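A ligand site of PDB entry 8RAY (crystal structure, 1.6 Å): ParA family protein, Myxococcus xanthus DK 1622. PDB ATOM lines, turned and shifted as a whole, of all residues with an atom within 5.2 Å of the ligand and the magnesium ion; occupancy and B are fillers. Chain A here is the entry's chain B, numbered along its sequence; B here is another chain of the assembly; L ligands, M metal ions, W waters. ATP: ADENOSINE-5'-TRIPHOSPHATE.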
ATOM      1  N   LYS A  12      12.733  -5.935  -7.209  1.00  0.00           N
ATOM      2  CA  LYS A  12      13.793  -6.290  -6.279  1.00  0.00           C
ATOM      3  C   LYS A  12      13.277  -7.287  -5.249  1.00  0.00           C
ATOM      4  O   LYS A  12      12.224  -7.088  -4.635  1.00  0.00           O
ATOM      5  CB  LYS A  12      14.344  -5.038  -5.585  1.00  0.00           C
ATOM      6  CG  LYS A  12      15.529  -5.287  -4.611  1.00  0.00           C
ATOM      7  CD  LYS A  12      16.792  -5.789  -5.331  1.00  0.00           C
ATOM      8  CE  LYS A  12      17.891  -6.222  -4.265  1.00  0.00           C
ATOM      9  NZ  LYS A  12      17.552  -7.511  -3.612  1.00  0.00           N
ATOM     10  N   GLY A  13      14.039  -8.350  -5.022  1.00  0.00           N
ATOM     11  CA  GLY A  13      13.604  -9.313  -4.021  1.00  0.00           C
ATOM     12  C   GLY A  13      13.755  -8.788  -2.588  1.00  0.00           C
ATOM     13  O   GLY A  13      14.755  -8.155  -2.247  1.00  0.00           O
ATOM     14  N   GLY A  14      12.760  -9.076  -1.741  1.00  0.00           N
ATOM     15  CA  GLY A  14      12.947  -8.888  -0.271  1.00  0.00           C
ATOM     16  C   GLY A  14      12.965  -7.438   0.185  1.00  0.00           C
ATOM     17  O   GLY A  14      13.835  -7.059   1.017  1.00  0.00           O
ATOM     18  N   VAL A  15      12.065  -6.599  -0.359  1.00  0.00           N
ATOM     19  CA  VAL A  15      11.962  -5.159  -0.081  1.00  0.00           C
ATOM     20  C   VAL A  15      10.736  -4.848   0.756  1.00  0.00           C
ATOM     21  O   VAL A  15      10.407  -3.657   0.932  1.00  0.00           O
ATOM     22  CB  VAL A  15      11.963  -4.307  -1.356  1.00  0.00           C
ATOM     23  CG1 VAL A  15      13.342  -4.493  -2.076  1.00  0.00           C
ATOM     24  CG2 VAL A  15      10.791  -4.715  -2.308  1.00  0.00           C
ATOM     25  N   GLY A  16      10.007  -5.860   1.222  1.00  0.00           N
ATOM     26  CA  GLY A  16       8.817  -5.584   2.026  1.00  0.00           C
ATOM     27  C   GLY A  16       7.475  -5.587   1.259  1.00  0.00           C
ATOM     28  O   GLY A  16       6.471  -5.049   1.777  1.00  0.00           O
ATOM     29  N   LYS A  17       7.433  -6.143   0.036  1.00  0.00           N
ATOM     30  CA  LYS A  17       6.157  -6.274  -0.678  1.00  0.00           C
ATOM     31  C   LYS A  17       5.107  -7.009   0.160  1.00  0.00           C
ATOM     32  O   LYS A  17       4.005  -6.493   0.374  1.00  0.00           O
ATOM     33  CB  LYS A  17       6.328  -7.031  -1.988  1.00  0.00           C
ATOM     34  CG  LYS A  17       7.105  -6.254  -3.056  1.00  0.00           C
ATOM     35  CD  LYS A  17       7.218  -7.041  -4.359  1.00  0.00           C
ATOM     36  CE  LYS A  17       8.067  -8.339  -4.271  1.00  0.00           C
ATOM     37  NZ  LYS A  17       9.539  -7.973  -4.029  1.00  0.00           N
ATOM     38  N   THR A  18       5.437  -8.232   0.578  1.00  0.00           N
ATOM     39  CA  THR A  18       4.483  -9.057   1.300  1.00  0.00           C
ATOM     40  C   THR A  18       4.189  -8.502   2.687  1.00  0.00           C
ATOM     41  O   THR A  18       3.037  -8.472   3.113  1.00  0.00           O
ATOM     42  CB  THR A  18       5.027 -10.482   1.380  1.00  0.00           C
ATOM     43  OG1 THR A  18       5.109 -11.011   0.047  1.00  0.00           O
ATOM     44  CG2 THR A  18       4.080 -11.378   2.294  1.00  0.00           C
ATOM     45  N   THR A  19       5.208  -8.031   3.390  1.00  0.00           N
ATOM     46  CA  THR A  19       4.972  -7.448   4.716  1.00  0.00           C
ATOM     47  C   THR A  19       4.023  -6.261   4.585  1.00  0.00           C
ATOM     48  O   THR A  19       3.123  -6.064   5.419  1.00  0.00           O
ATOM     49  CB  THR A  19       6.339  -7.053   5.304  1.00  0.00           C
ATOM     50  OG1 THR A  19       7.126  -8.224   5.523  1.00  0.00           O
ATOM     51  CG2 THR A  19       6.184  -6.360   6.702  1.00  0.00           C
ATOM     52  N   THR A  20       4.175  -5.483   3.528  1.00  0.00           N
ATOM     53  CA  THR A  20       3.267  -4.365   3.291  1.00  0.00           C
ATOM     54  C   THR A  20       1.874  -4.847   2.888  1.00  0.00           C
ATOM     55  O   THR A  20       0.873  -4.349   3.400  1.00  0.00           O
ATOM     56  CB  THR A  20       3.877  -3.445   2.220  1.00  0.00           C
ATOM     57  OG1 THR A  20       5.130  -2.892   2.706  1.00  0.00           O
ATOM     58  CG2 THR A  20       2.923  -2.324   1.805  1.00  0.00           C
ATOM     59  N   GLN A  43       5.758 -18.070  -4.348  1.00  0.00           N
ATOM     60  CA  GLN A  43       6.220 -18.317  -2.983  1.00  0.00           C
ATOM     61  C   GLN A  43       5.092 -18.315  -1.984  1.00  0.00           C
ATOM     62  O   GLN A  43       5.249 -18.938  -0.946  1.00  0.00           O
ATOM     63  CB  GLN A  43       7.250 -17.238  -2.567  1.00  0.00           C
ATOM     64  CG  GLN A  43       8.519 -17.150  -3.515  1.00  0.00           C
ATOM     65  CD  GLN A  43       8.355 -16.179  -4.671  1.00  0.00           C
ATOM     66  OE1 GLN A  43       7.242 -15.851  -5.128  1.00  0.00           O
ATOM     67  NE2 GLN A  43       9.487 -15.739  -5.202  1.00  0.00           N
ATOM     68  N   ASN A  45       3.842 -16.144   0.160  1.00  0.00           N
ATOM     69  CA  ASN A  45       4.143 -15.595   1.516  1.00  0.00           C
ATOM     70  C   ASN A  45       2.956 -14.792   2.089  1.00  0.00           C
ATOM     71  O   ASN A  45       2.788 -14.772   3.293  1.00  0.00           O
ATOM     72  CB  ASN A  45       5.431 -14.787   1.495  1.00  0.00           C
ATOM     73  CG  ASN A  45       6.662 -15.610   1.190  1.00  0.00           C
ATOM     74  OD1 ASN A  45       6.654 -16.836   1.313  1.00  0.00           O
ATOM     75  ND2 ASN A  45       7.733 -14.950   0.799  1.00  0.00           N
ATOM     76  N   ASP A 126      -0.472  -8.883  -4.030  1.00  0.00           N
ATOM     77  CA  ASP A 126       0.938  -9.041  -3.665  1.00  0.00           C
ATOM     78  C   ASP A 126       1.659  -9.653  -4.852  1.00  0.00           C
ATOM     79  O   ASP A 126       1.231 -10.680  -5.363  1.00  0.00           O
ATOM     80  CB  ASP A 126       1.100  -9.948  -2.440  1.00  0.00           C
ATOM     81  CG  ASP A 126       2.503  -9.965  -1.892  1.00  0.00           C
ATOM     82  OD1 ASP A 126       3.288  -9.037  -2.185  1.00  0.00           O
ATOM     83  OD2 ASP A 126       2.807 -10.879  -1.098  1.00  0.00           O
ATOM     84  N   CYS A 127       2.707  -9.021  -5.306  1.00  0.00           N
ATOM     85  CA  CYS A 127       3.383  -9.470  -6.539  1.00  0.00           C
ATOM     86  C   CYS A 127       4.690 -10.164  -6.172  1.00  0.00           C
ATOM     87  O   CYS A 127       5.386  -9.761  -5.249  1.00  0.00           O
ATOM     88  CB  CYS A 127       3.776  -8.306  -7.439  1.00  0.00           C
ATOM     89  SG  CYS A 127       2.315  -7.471  -8.130  1.00  0.00           S
ATOM     90  N   PRO A 128       5.125 -11.115  -7.001  1.00  0.00           N
ATOM     91  CA  PRO A 128       6.475 -11.689  -6.820  1.00  0.00           C
ATOM     92  C   PRO A 128       7.541 -10.698  -7.282  1.00  0.00           C
ATOM     93  O   PRO A 128       7.257  -9.705  -7.975  1.00  0.00           O
ATOM     94  CB  PRO A 128       6.436 -12.940  -7.707  1.00  0.00           C
ATOM     95  CG  PRO A 128       5.448 -12.552  -8.836  1.00  0.00           C
ATOM     96  CD  PRO A 128       4.408 -11.656  -8.172  1.00  0.00           C
ATOM     97  N   PRO A 129       8.797 -10.955  -6.927  1.00  0.00           N
ATOM     98  CA  PRO A 129       9.966 -10.126  -7.336  1.00  0.00           C
ATOM     99  C   PRO A 129      10.347 -10.415  -8.781  1.00  0.00           C
ATOM    100  O   PRO A 129      11.358 -11.063  -9.071  1.00  0.00           O
ATOM    101  CB  PRO A 129      11.060 -10.574  -6.364  1.00  0.00           C
ATOM    102  CG  PRO A 129      10.712 -12.065  -6.054  1.00  0.00           C
ATOM    103  CD  PRO A 129       9.147 -12.078  -6.028  1.00  0.00           C
ATOM    104  N   MET A 186      11.768  -0.785   5.549  1.00  0.00           N
ATOM    105  CA  MET A 186      12.955  -1.442   6.081  1.00  0.00           C
ATOM    106  C   MET A 186      14.044  -0.400   6.367  1.00  0.00           C
ATOM    107  O   MET A 186      15.210  -0.563   6.050  1.00  0.00           O
ATOM    108  CB  MET A 186      13.402  -2.531   5.079  1.00  0.00           C
ATOM    109  CG  MET A 186      12.222  -3.536   4.849  1.00  0.00           C
ATOM    110  SD  MET A 186      12.728  -4.779   3.601  1.00  0.00           S
ATOM    111  CE  MET A 186      13.745  -5.819   4.591  1.00  0.00           C
ATOM    112  N   VAL A 214       8.426   2.904   7.040  1.00  0.00           N
ATOM    113  CA  VAL A 214       8.357   1.660   7.846  1.00  0.00           C
ATOM    114  C   VAL A 214       9.773   1.367   8.325  1.00  0.00           C
ATOM    115  O   VAL A 214      10.669   1.160   7.505  1.00  0.00           O
ATOM    116  CB  VAL A 214       7.772   0.470   7.072  1.00  0.00           C
ATOM    117  CG1 VAL A 214       7.629  -0.741   7.971  1.00  0.00           C
ATOM    118  CG2 VAL A 214       6.447   0.822   6.417  1.00  0.00           C
ATOM    119  N   PRO A 215       9.993   1.340   9.645  1.00  0.00           N
ATOM    120  CA  PRO A 215      11.310   1.080  10.138  1.00  0.00           C
ATOM    121  C   PRO A 215      11.645  -0.400  10.248  1.00  0.00           C
ATOM    122  O   PRO A 215      10.739  -1.187  10.366  1.00  0.00           O
ATOM    123  CB  PRO A 215      11.186   1.618  11.576  1.00  0.00           C
ATOM    124  CG  PRO A 215       9.756   1.331  11.962  1.00  0.00           C
ATOM    125  CD  PRO A 215       8.990   1.568  10.682  1.00  0.00           C
ATOM    126  N   ARG A 216      12.919  -0.730  10.092  1.00  0.00           N
ATOM    127  CA  ARG A 216      13.310  -2.087  10.446  1.00  0.00           C
ATOM    128  C   ARG A 216      12.828  -2.388  11.854  1.00  0.00           C
ATOM    129  O   ARG A 216      13.094  -1.622  12.805  1.00  0.00           O
ATOM    130  CB  ARG A 216      14.834  -2.266  10.384  1.00  0.00           C
ATOM    131  CG  ARG A 216      15.472  -2.068   9.021  1.00  0.00           C
ATOM    132  CD  ARG A 216      16.868  -2.760   8.914  1.00  0.00           C
ATOM    133  NE  ARG A 216      16.752  -4.166   9.279  1.00  0.00           N
ATOM    134  CZ  ARG A 216      16.505  -5.149   8.392  1.00  0.00           C
ATOM    135  NH1 ARG A 216      16.347  -4.896   7.095  1.00  0.00           N
ATOM    136  NH2 ARG A 216      16.413  -6.405   8.817  1.00  0.00           N
ATOM    137  N   ASN A 217      12.185  -3.541  12.039  1.00  0.00           N
ATOM    138  CA  ASN A 217      11.592  -3.867  13.334  1.00  0.00           C
ATOM    139  C   ASN A 217      11.508  -5.381  13.459  1.00  0.00           C
ATOM    140  O   ASN A 217      10.942  -6.043  12.590  1.00  0.00           O
ATOM    141  CB  ASN A 217      10.210  -3.203  13.439  1.00  0.00           C
ATOM    142  CG  ASN A 217       9.520  -3.505  14.749  1.00  0.00           C
ATOM    143  OD1 ASN A 217       9.020  -4.601  14.954  1.00  0.00           O
ATOM    144  ND2 ASN A 217       9.580  -2.553  15.676  1.00  0.00           N
ATOM    145  N   VAL A 218      12.131  -5.940  14.501  1.00  0.00           N
ATOM    146  CA  VAL A 218      12.285  -7.393  14.585  1.00  0.00           C
ATOM    147  C   VAL A 218      10.931  -8.079  14.650  1.00  0.00           C
ATOM    148  O   VAL A 218      10.740  -9.138  14.065  1.00  0.00           O
ATOM    149  CB  VAL A 218      13.149  -7.778  15.809  1.00  0.00           C
ATOM    150  CG1 VAL A 218      13.107  -9.291  16.004  1.00  0.00           C
ATOM    151  CG2 VAL A 218      14.654  -7.261  15.701  1.00  0.00           C
ATOM    152  N   LEU A 220       8.269  -7.306  13.139  1.00  0.00           N
ATOM    153  CA  LEU A 220       7.608  -7.438  11.840  1.00  0.00           C
ATOM    154  C   LEU A 220       8.069  -8.701  11.159  1.00  0.00           C
ATOM    155  O   LEU A 220       7.340  -9.259  10.334  1.00  0.00           O
ATOM    156  CB  LEU A 220       7.900  -6.241  10.923  1.00  0.00           C
ATOM    157  CG  LEU A 220       7.050  -5.003  11.061  1.00  0.00           C
ATOM    158  CD1 LEU A 220       7.635  -3.904  10.197  1.00  0.00           C
ATOM    159  CD2 LEU A 220       5.582  -5.261  10.717  1.00  0.00           C
ATOM    160  N   SER A 221       9.311  -9.098  11.407  1.00  0.00           N
ATOM    161  CA  SER A 221       9.842 -10.286  10.764  1.00  0.00           C
ATOM    162  C   SER A 221       9.424 -11.556  11.469  1.00  0.00           C
ATOM    163  O   SER A 221       9.465 -12.627  10.854  1.00  0.00           O
ATOM    164  CB  SER A 221      11.364 -10.213  10.661  1.00  0.00           C
ATOM    165  OG  SER A 221      11.943 -10.423  11.928  1.00  0.00           O
ATOM    166  N   PRO A 224       4.973 -13.387  10.861  1.00  0.00           N
ATOM    167  CA  PRO A 224       4.502 -14.394   9.885  1.00  0.00           C
ATOM    168  C   PRO A 224       4.714 -15.827  10.357  1.00  0.00           C
ATOM    169  O   PRO A 224       3.961 -16.725   9.933  1.00  0.00           O
ATOM    170  CB  PRO A 224       5.363 -14.149   8.641  1.00  0.00           C
ATOM    171  CG  PRO A 224       6.012 -12.865   8.841  1.00  0.00           C
ATOM    172  CD  PRO A 224       5.981 -12.473  10.290  1.00  0.00           C
ATOM    173  N   GLN B  11      14.603 -18.940  -4.671  1.00  0.00           N
ATOM    174  CA  GLN B  11      13.506 -18.146  -5.226  1.00  0.00           C
ATOM    175  C   GLN B  11      12.953 -17.118  -4.237  1.00  0.00           C
ATOM    176  O   GLN B  11      12.219 -16.223  -4.684  1.00  0.00           O
ATOM    177  CB  GLN B  11      12.385 -19.093  -5.729  1.00  0.00           C
ATOM    178  CG  GLN B  11      11.535 -19.789  -4.597  1.00  0.00           C
ATOM    179  CD  GLN B  11      12.200 -21.079  -4.094  1.00  0.00           C
ATOM    180  OE1 GLN B  11      13.389 -21.312  -4.259  1.00  0.00           O
ATOM    181  NE2 GLN B  11      11.414 -21.920  -3.472  1.00  0.00           N
ATOM    182  N   LYS B  12      13.278 -17.219  -2.931  1.00  0.00           N
ATOM    183  CA  LYS B  12      12.875 -16.147  -2.011  1.00  0.00           C
ATOM    184  C   LYS B  12      13.655 -14.875  -2.344  1.00  0.00           C
ATOM    185  O   LYS B  12      14.880 -14.900  -2.529  1.00  0.00           O
ATOM    186  CB  LYS B  12      13.084 -16.555  -0.552  1.00  0.00           C
ATOM    187  CG  LYS B  12      12.737 -15.438   0.460  1.00  0.00           C
ATOM    188  CD  LYS B  12      11.185 -15.284   0.525  1.00  0.00           C
ATOM    189  CE  LYS B  12      10.830 -14.119   1.512  1.00  0.00           C
ATOM    190  NZ  LYS B  12      11.159 -12.759   0.887  1.00  0.00           N
ATOM    191  N   GLY B  13      12.945 -13.744  -2.427  1.00  0.00           N
ATOM    192  CA  GLY B  13      13.638 -12.498  -2.743  1.00  0.00           C
ATOM    193  C   GLY B  13      14.452 -11.959  -1.580  1.00  0.00           C
ATOM    194  O   GLY B  13      14.021 -11.988  -0.412  1.00  0.00           O
ATOM    195  N   GLN B 150      18.472 -17.053   4.091  1.00  0.00           N
ATOM    196  CA  GLN B 150      18.282 -16.030   5.103  1.00  0.00           C
ATOM    197  C   GLN B 150      17.664 -16.615   6.375  1.00  0.00           C
ATOM    198  O   GLN B 150      16.705 -17.410   6.320  1.00  0.00           O
ATOM    199  CB  GLN B 150      17.416 -14.900   4.540  1.00  0.00           C
ATOM    200  CG  GLN B 150      17.038 -13.848   5.583  1.00  0.00           C
ATOM    201  CD  GLN B 150      16.104 -12.821   5.029  1.00  0.00           C
ATOM    202  OE1 GLN B 150      15.217 -13.141   4.230  1.00  0.00           O
ATOM    203  NE2 GLN B 150      16.267 -11.561   5.448  1.00  0.00           N
ATOM    204  N   GLU B 152      15.473 -16.107   8.499  1.00  0.00           N
ATOM    205  CA  GLU B 152      14.153 -15.574   8.824  1.00  0.00           C
ATOM    206  C   GLU B 152      13.112 -16.558   8.314  1.00  0.00           C
ATOM    207  O   GLU B 152      13.398 -17.490   7.556  1.00  0.00           O
ATOM    208  CB  GLU B 152      13.904 -14.164   8.207  1.00  0.00           C
ATOM    209  CG  GLU B 152      14.842 -13.134   8.798  1.00  0.00           C
ATOM    210  CD  GLU B 152      14.561 -11.685   8.474  1.00  0.00           C
ATOM    211  OE1 GLU B 152      13.574 -11.352   7.853  1.00  0.00           O
ATOM    212  OE2 GLU B 152      15.381 -10.827   8.862  1.00  0.00           O
ATOM    213  N   TYR B 153      11.864 -16.322   8.722  1.00  0.00           N
ATOM    214  CA  TYR B 153      10.807 -17.302   8.557  1.00  0.00           C
ATOM    215  C   TYR B 153      10.490 -17.604   7.101  1.00  0.00           C
ATOM    216  O   TYR B 153      10.452 -18.780   6.696  1.00  0.00           O
ATOM    217  CB  TYR B 153       9.566 -16.826   9.292  1.00  0.00           C
ATOM    218  CG  TYR B 153       8.434 -17.783   9.036  1.00  0.00           C
ATOM    219  CD1 TYR B 153       8.439 -19.032   9.659  1.00  0.00           C
ATOM    220  CD2 TYR B 153       7.431 -17.465   8.174  1.00  0.00           C
ATOM    221  CE1 TYR B 153       7.442 -19.934   9.404  1.00  0.00           C
ATOM    222  CE2 TYR B 153       6.440 -18.347   7.892  1.00  0.00           C
ATOM    223  CZ  TYR B 153       6.452 -19.585   8.532  1.00  0.00           C
ATOM    224  OH  TYR B 153       5.450 -20.487   8.291  1.00  0.00           O
ATOM    225  N   TYR B 154      10.161 -16.574   6.292  1.00  0.00           N
ATOM    226  CA  TYR B 154       9.701 -16.896   4.931  1.00  0.00           C
ATOM    227  C   TYR B 154      10.781 -17.657   4.157  1.00  0.00           C
ATOM    228  O   TYR B 154      10.453 -18.587   3.406  1.00  0.00           O
ATOM    229  CB  TYR B 154       9.332 -15.637   4.165  1.00  0.00           C
ATOM    230  CG  TYR B 154       8.001 -15.011   4.548  1.00  0.00           C
ATOM    231  CD1 TYR B 154       6.860 -15.780   4.840  1.00  0.00           C
ATOM    232  CD2 TYR B 154       7.893 -13.637   4.565  1.00  0.00           C
ATOM    233  CE1 TYR B 154       5.656 -15.164   5.183  1.00  0.00           C
ATOM    234  CE2 TYR B 154       6.696 -13.009   4.902  1.00  0.00           C
ATOM    235  CZ  TYR B 154       5.600 -13.780   5.197  1.00  0.00           C
ATOM    236  OH  TYR B 154       4.430 -13.131   5.477  1.00  0.00           O
HETATM  237  PG  ATP L   1       9.854 -11.230  -2.139  1.00  0.00           P
HETATM  238  O1G ATP L   1       8.397 -11.312  -2.445  1.00  0.00           O
HETATM  239  O2G ATP L   1      10.623 -10.452  -3.149  1.00  0.00           O
HETATM  240  O3G ATP L   1      10.464 -12.560  -1.826  1.00  0.00           O
HETATM  241  PB  ATP L   1       9.113  -9.107  -0.334  1.00  0.00           P
HETATM  242  O1B ATP L   1       9.443  -7.940  -1.176  1.00  0.00           O
HETATM  243  O2B ATP L   1       7.696  -9.536  -0.220  1.00  0.00           O
HETATM  244  O3B ATP L   1       9.978 -10.358  -0.794  1.00  0.00           O
HETATM  245  PA  ATP L   1       9.270  -9.517   2.511  1.00  0.00           P
HETATM  246  O1A ATP L   1       8.015  -8.892   3.016  1.00  0.00           O
HETATM  247  O2A ATP L   1       9.314 -10.992   2.338  1.00  0.00           O
HETATM  248  O3A ATP L   1       9.673  -8.842   1.133  1.00  0.00           O
HETATM  249  O5' ATP L   1      10.478  -9.052   3.441  1.00  0.00           O
HETATM  250  C5' ATP L   1      11.738  -9.747   3.348  1.00  0.00           C
HETATM  251  C4' ATP L   1      12.110 -10.274   4.709  1.00  0.00           C
HETATM  252  O4' ATP L   1      12.319  -9.155   5.607  1.00  0.00           O
HETATM  253  C3' ATP L   1      11.065 -11.160   5.379  1.00  0.00           C
HETATM  254  O3' ATP L   1      11.716 -12.187   6.118  1.00  0.00           O
HETATM  255  C2' ATP L   1      10.287 -10.167   6.248  1.00  0.00           C
HETATM  256  O2' ATP L   1       9.686 -10.777   7.374  1.00  0.00           O
HETATM  257  C1' ATP L   1      11.369  -9.171   6.652  1.00  0.00           C
HETATM  258  N9  ATP L   1      10.901  -7.813   6.800  1.00  0.00           N
HETATM  259  C8  ATP L   1      10.115  -7.111   5.940  1.00  0.00           C
HETATM  260  N7  ATP L   1       9.898  -5.879   6.336  1.00  0.00           N
HETATM  261  C5  ATP L   1      10.601  -5.766   7.523  1.00  0.00           C
HETATM  262  C6  ATP L   1      10.770  -4.704   8.433  1.00  0.00           C
HETATM  263  N6  ATP L   1      10.250  -3.494   8.261  1.00  0.00           N
HETATM  264  N1  ATP L   1      11.548  -4.929   9.521  1.00  0.00           N
HETATM  265  C2  ATP L   1      12.088  -6.147   9.664  1.00  0.00           C
HETATM  266  N3  ATP L   1      11.992  -7.220   8.888  1.00  0.00           N
HETATM  267  C4  ATP L   1      11.227  -6.952   7.822  1.00  0.00           C
HETATM  268 MG    MG M   1       6.852 -11.238  -1.138  1.00  0.00          MG
HETATM  269  O   HOH W   1       9.974 -13.854   7.462  1.00  0.00           O
HETATM  270  O   HOH W   2       5.736 -10.235  -2.541  1.00  0.00           O
HETATM  271  O   HOH W   3      13.685 -11.986   2.262  1.00  0.00           O
HETATM  272  O   HOH W   4       7.735 -12.242   0.461  1.00  0.00           O
HETATM  273  O   HOH W   5      15.295  -9.037   4.887  1.00  0.00           O
HETATM  274  O   HOH W   6       7.100  -9.933   7.440  1.00  0.00           O
HETATM  275  O   HOH W   7       6.153 -13.075  -1.849  1.00  0.00           O
HETATM  276  O   HOH W   8       8.775  -3.220   5.757  1.00  0.00           O
HETATM  277  O   HOH W   9       8.467 -14.548  -1.929  1.00  0.00           O
HETATM  278  O   HOH W  10      12.717 -14.434   4.787  1.00  0.00           O
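Water W2 lies within hydrogen-bond range of the side-chain carboxylate of Asp 126 (2.7 Å) and the backbone carbonyl oxygen of Cys 127 (2.8 Å).
Water W4 lies within hydrogen-bond range of the side-chain amide nitrogen (ND2) of Asn 45 (2.7 Å), an oxygen (O2A) of the ligand (2.8 Å) and the side-chain amino group (NZ) of Lys 12 of chain B (3.5 Å).
Water W10 bridges an oxygen (O3') of the ligand and the side-chain amide oxygen (OE1) of Gln 150 of chain B.
Water W9 lies within hydrogen-bond range of an oxygen (O3G) of the ligand and the side-chain amide nitrogen (ND2) of Asn 45.
Water W5 lies within hydrogen-bond range of NE2 of Gln 150 of chain B (2.8 Å) and O4' of the ligand (3.1 Å).
Water W3 lies within hydrogen-bond range of the backbone carbonyl oxygen of Gly 13 of chain B (2.7 Å), the side-chain amide oxygen of Gln 150 of chain B (2.7 Å) and the side-chain amino group of Lys 12 of chain B (3.0 Å).
One residue has an atom within 4 Å of the magnesium ion: Thr 18.
The nearest printed residue that does not touch the magnesium ion is Asp 126 (4.1 Å).
An oxygen (O2B) of the ligand lies close to the backbone NH (N) of Thr 18, at 2.7 Å.
OE1 of Glu 152 of chain B is in hydrogen-bond range of O3' of the ligand.
An oxygen (O1A) of the ligand sits at hydrogen-bond distance from the backbone NH (N) of Thr 19 (3.0 Å).
The side-chain hydroxyl of Thr 19 lies within hydrogen-bond range of an oxygen (O1A) of the ligand, at 2.7 Å.
NZ of Lys 12 of chain B is in salt-bridge range of O3G of the ligand, at 2.8 Å.
N of Gly 13 of chain B lies within hydrogen-bond range of O3G of the ligand (2.8 Å).
The backbone NH (N) of Lys 17 lies within hydrogen-bond range of an oxygen (O1B) of the ligand.
The side-chain amino group of Lys 17 lies within salt-bridge range of an oxygen (O2G) of the ligand (2.8 Å).
O2G of the ligand is in hydrogen-bond range of N of Gly 14.
N of Asn 217 sits at hydrogen-bond distance from N1 of the ligand (2.9 Å).
N of Gly 16 lies within hydrogen-bond range of O3A of the ligand (3.0 Å).
The backbone NH (N) of Val 15 lies within hydrogen-bond range of an oxygen (O1B) of the ligand (3.1 Å).
The backbone carbonyl oxygen of Pro 215 sits at hydrogen-bond distance from a nitrogen (N6) of the ligand (3.2 Å).
O1G of the ligand binds the magnesium ion, 2.0 Å away.
Water W2 is bound to the magnesium ion (2.1 Å).
Water W4 is bound to the magnesium ion (2.1 Å).
Water W7 binds the magnesium ion (2.1 Å).
The magnesium ion is bound by O2B of the ligand (2.1 Å).
OG1 of Thr 18 binds the magnesium ion, 2.1 Å away.
CA of Gly 13 of chain A touches O2G of the ligand, at 3.3 Å.
Pro 129 touches the ligand (CB to O2G, 3.2 Å).
Met 186 touches the ligand (CG to N7, 3.6 Å).
Val 214 touches the ligand.
Arg 216 touches the ligand.
Leu 220 touches the ligand.
CA of Ser 221 touches O2' of the ligand, at 3.4 Å.
Tyr 154 of chain B touches the ligand (CD2 to O2A, 3.7 Å).
Hydrophobic or aromatic side chains within 4 Å of the ligand: Val 15, Pro 129, Met 186, Val 214, Leu 220 and Tyr 154 of chain B.
Within 4 Å of the ligand: Gly 13 of chain A, Gly 14, Val 15, Gly 16, Lys 17, Thr 18, Thr 19, Pro 129, Met 186, Val 214, Pro 215, Arg 216, Asn 217, Leu 220, Ser 221, Lys 12 of chain B, Gly 13 of chain B, Glu 152 of chain B and Tyr 154 of chain B.
The nearest printed residue that does not touch the ligand is Lys 12 of chain A (4.01 Å).
The side-chain hydroxyl of Thr 18 lies close to the side-chain carboxylate of Asp 126, at 2.6 Å.
The backbone NH of Gly 14 sits close to the backbone carbonyl oxygen of Gly 13 of chain B.
NZ of Lys 17 sits at hydrogen-bond distance from O of Lys 12 of chain A.
OD1 of Asn 217 lies within hydrogen-bond range of N of Leu 220 (3.3 Å).
O of Gly 16 sits at hydrogen-bond distance from OG1 of Thr 20, at 2.7 Å.
The side-chain hydroxyl (OG) of Ser 221 is in hydrogen-bond range of the backbone carbonyl oxygen (O) of Val 218.
The backbone NH (N) of Met 186 is in hydrogen-bond range of the backbone carbonyl oxygen (O) of Val 214 (3.0 Å).
The side-chain hydroxyl of Tyr 154 of chain B is in hydrogen-bond range of the backbone carbonyl oxygen of Asn 45 (3.2 Å).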
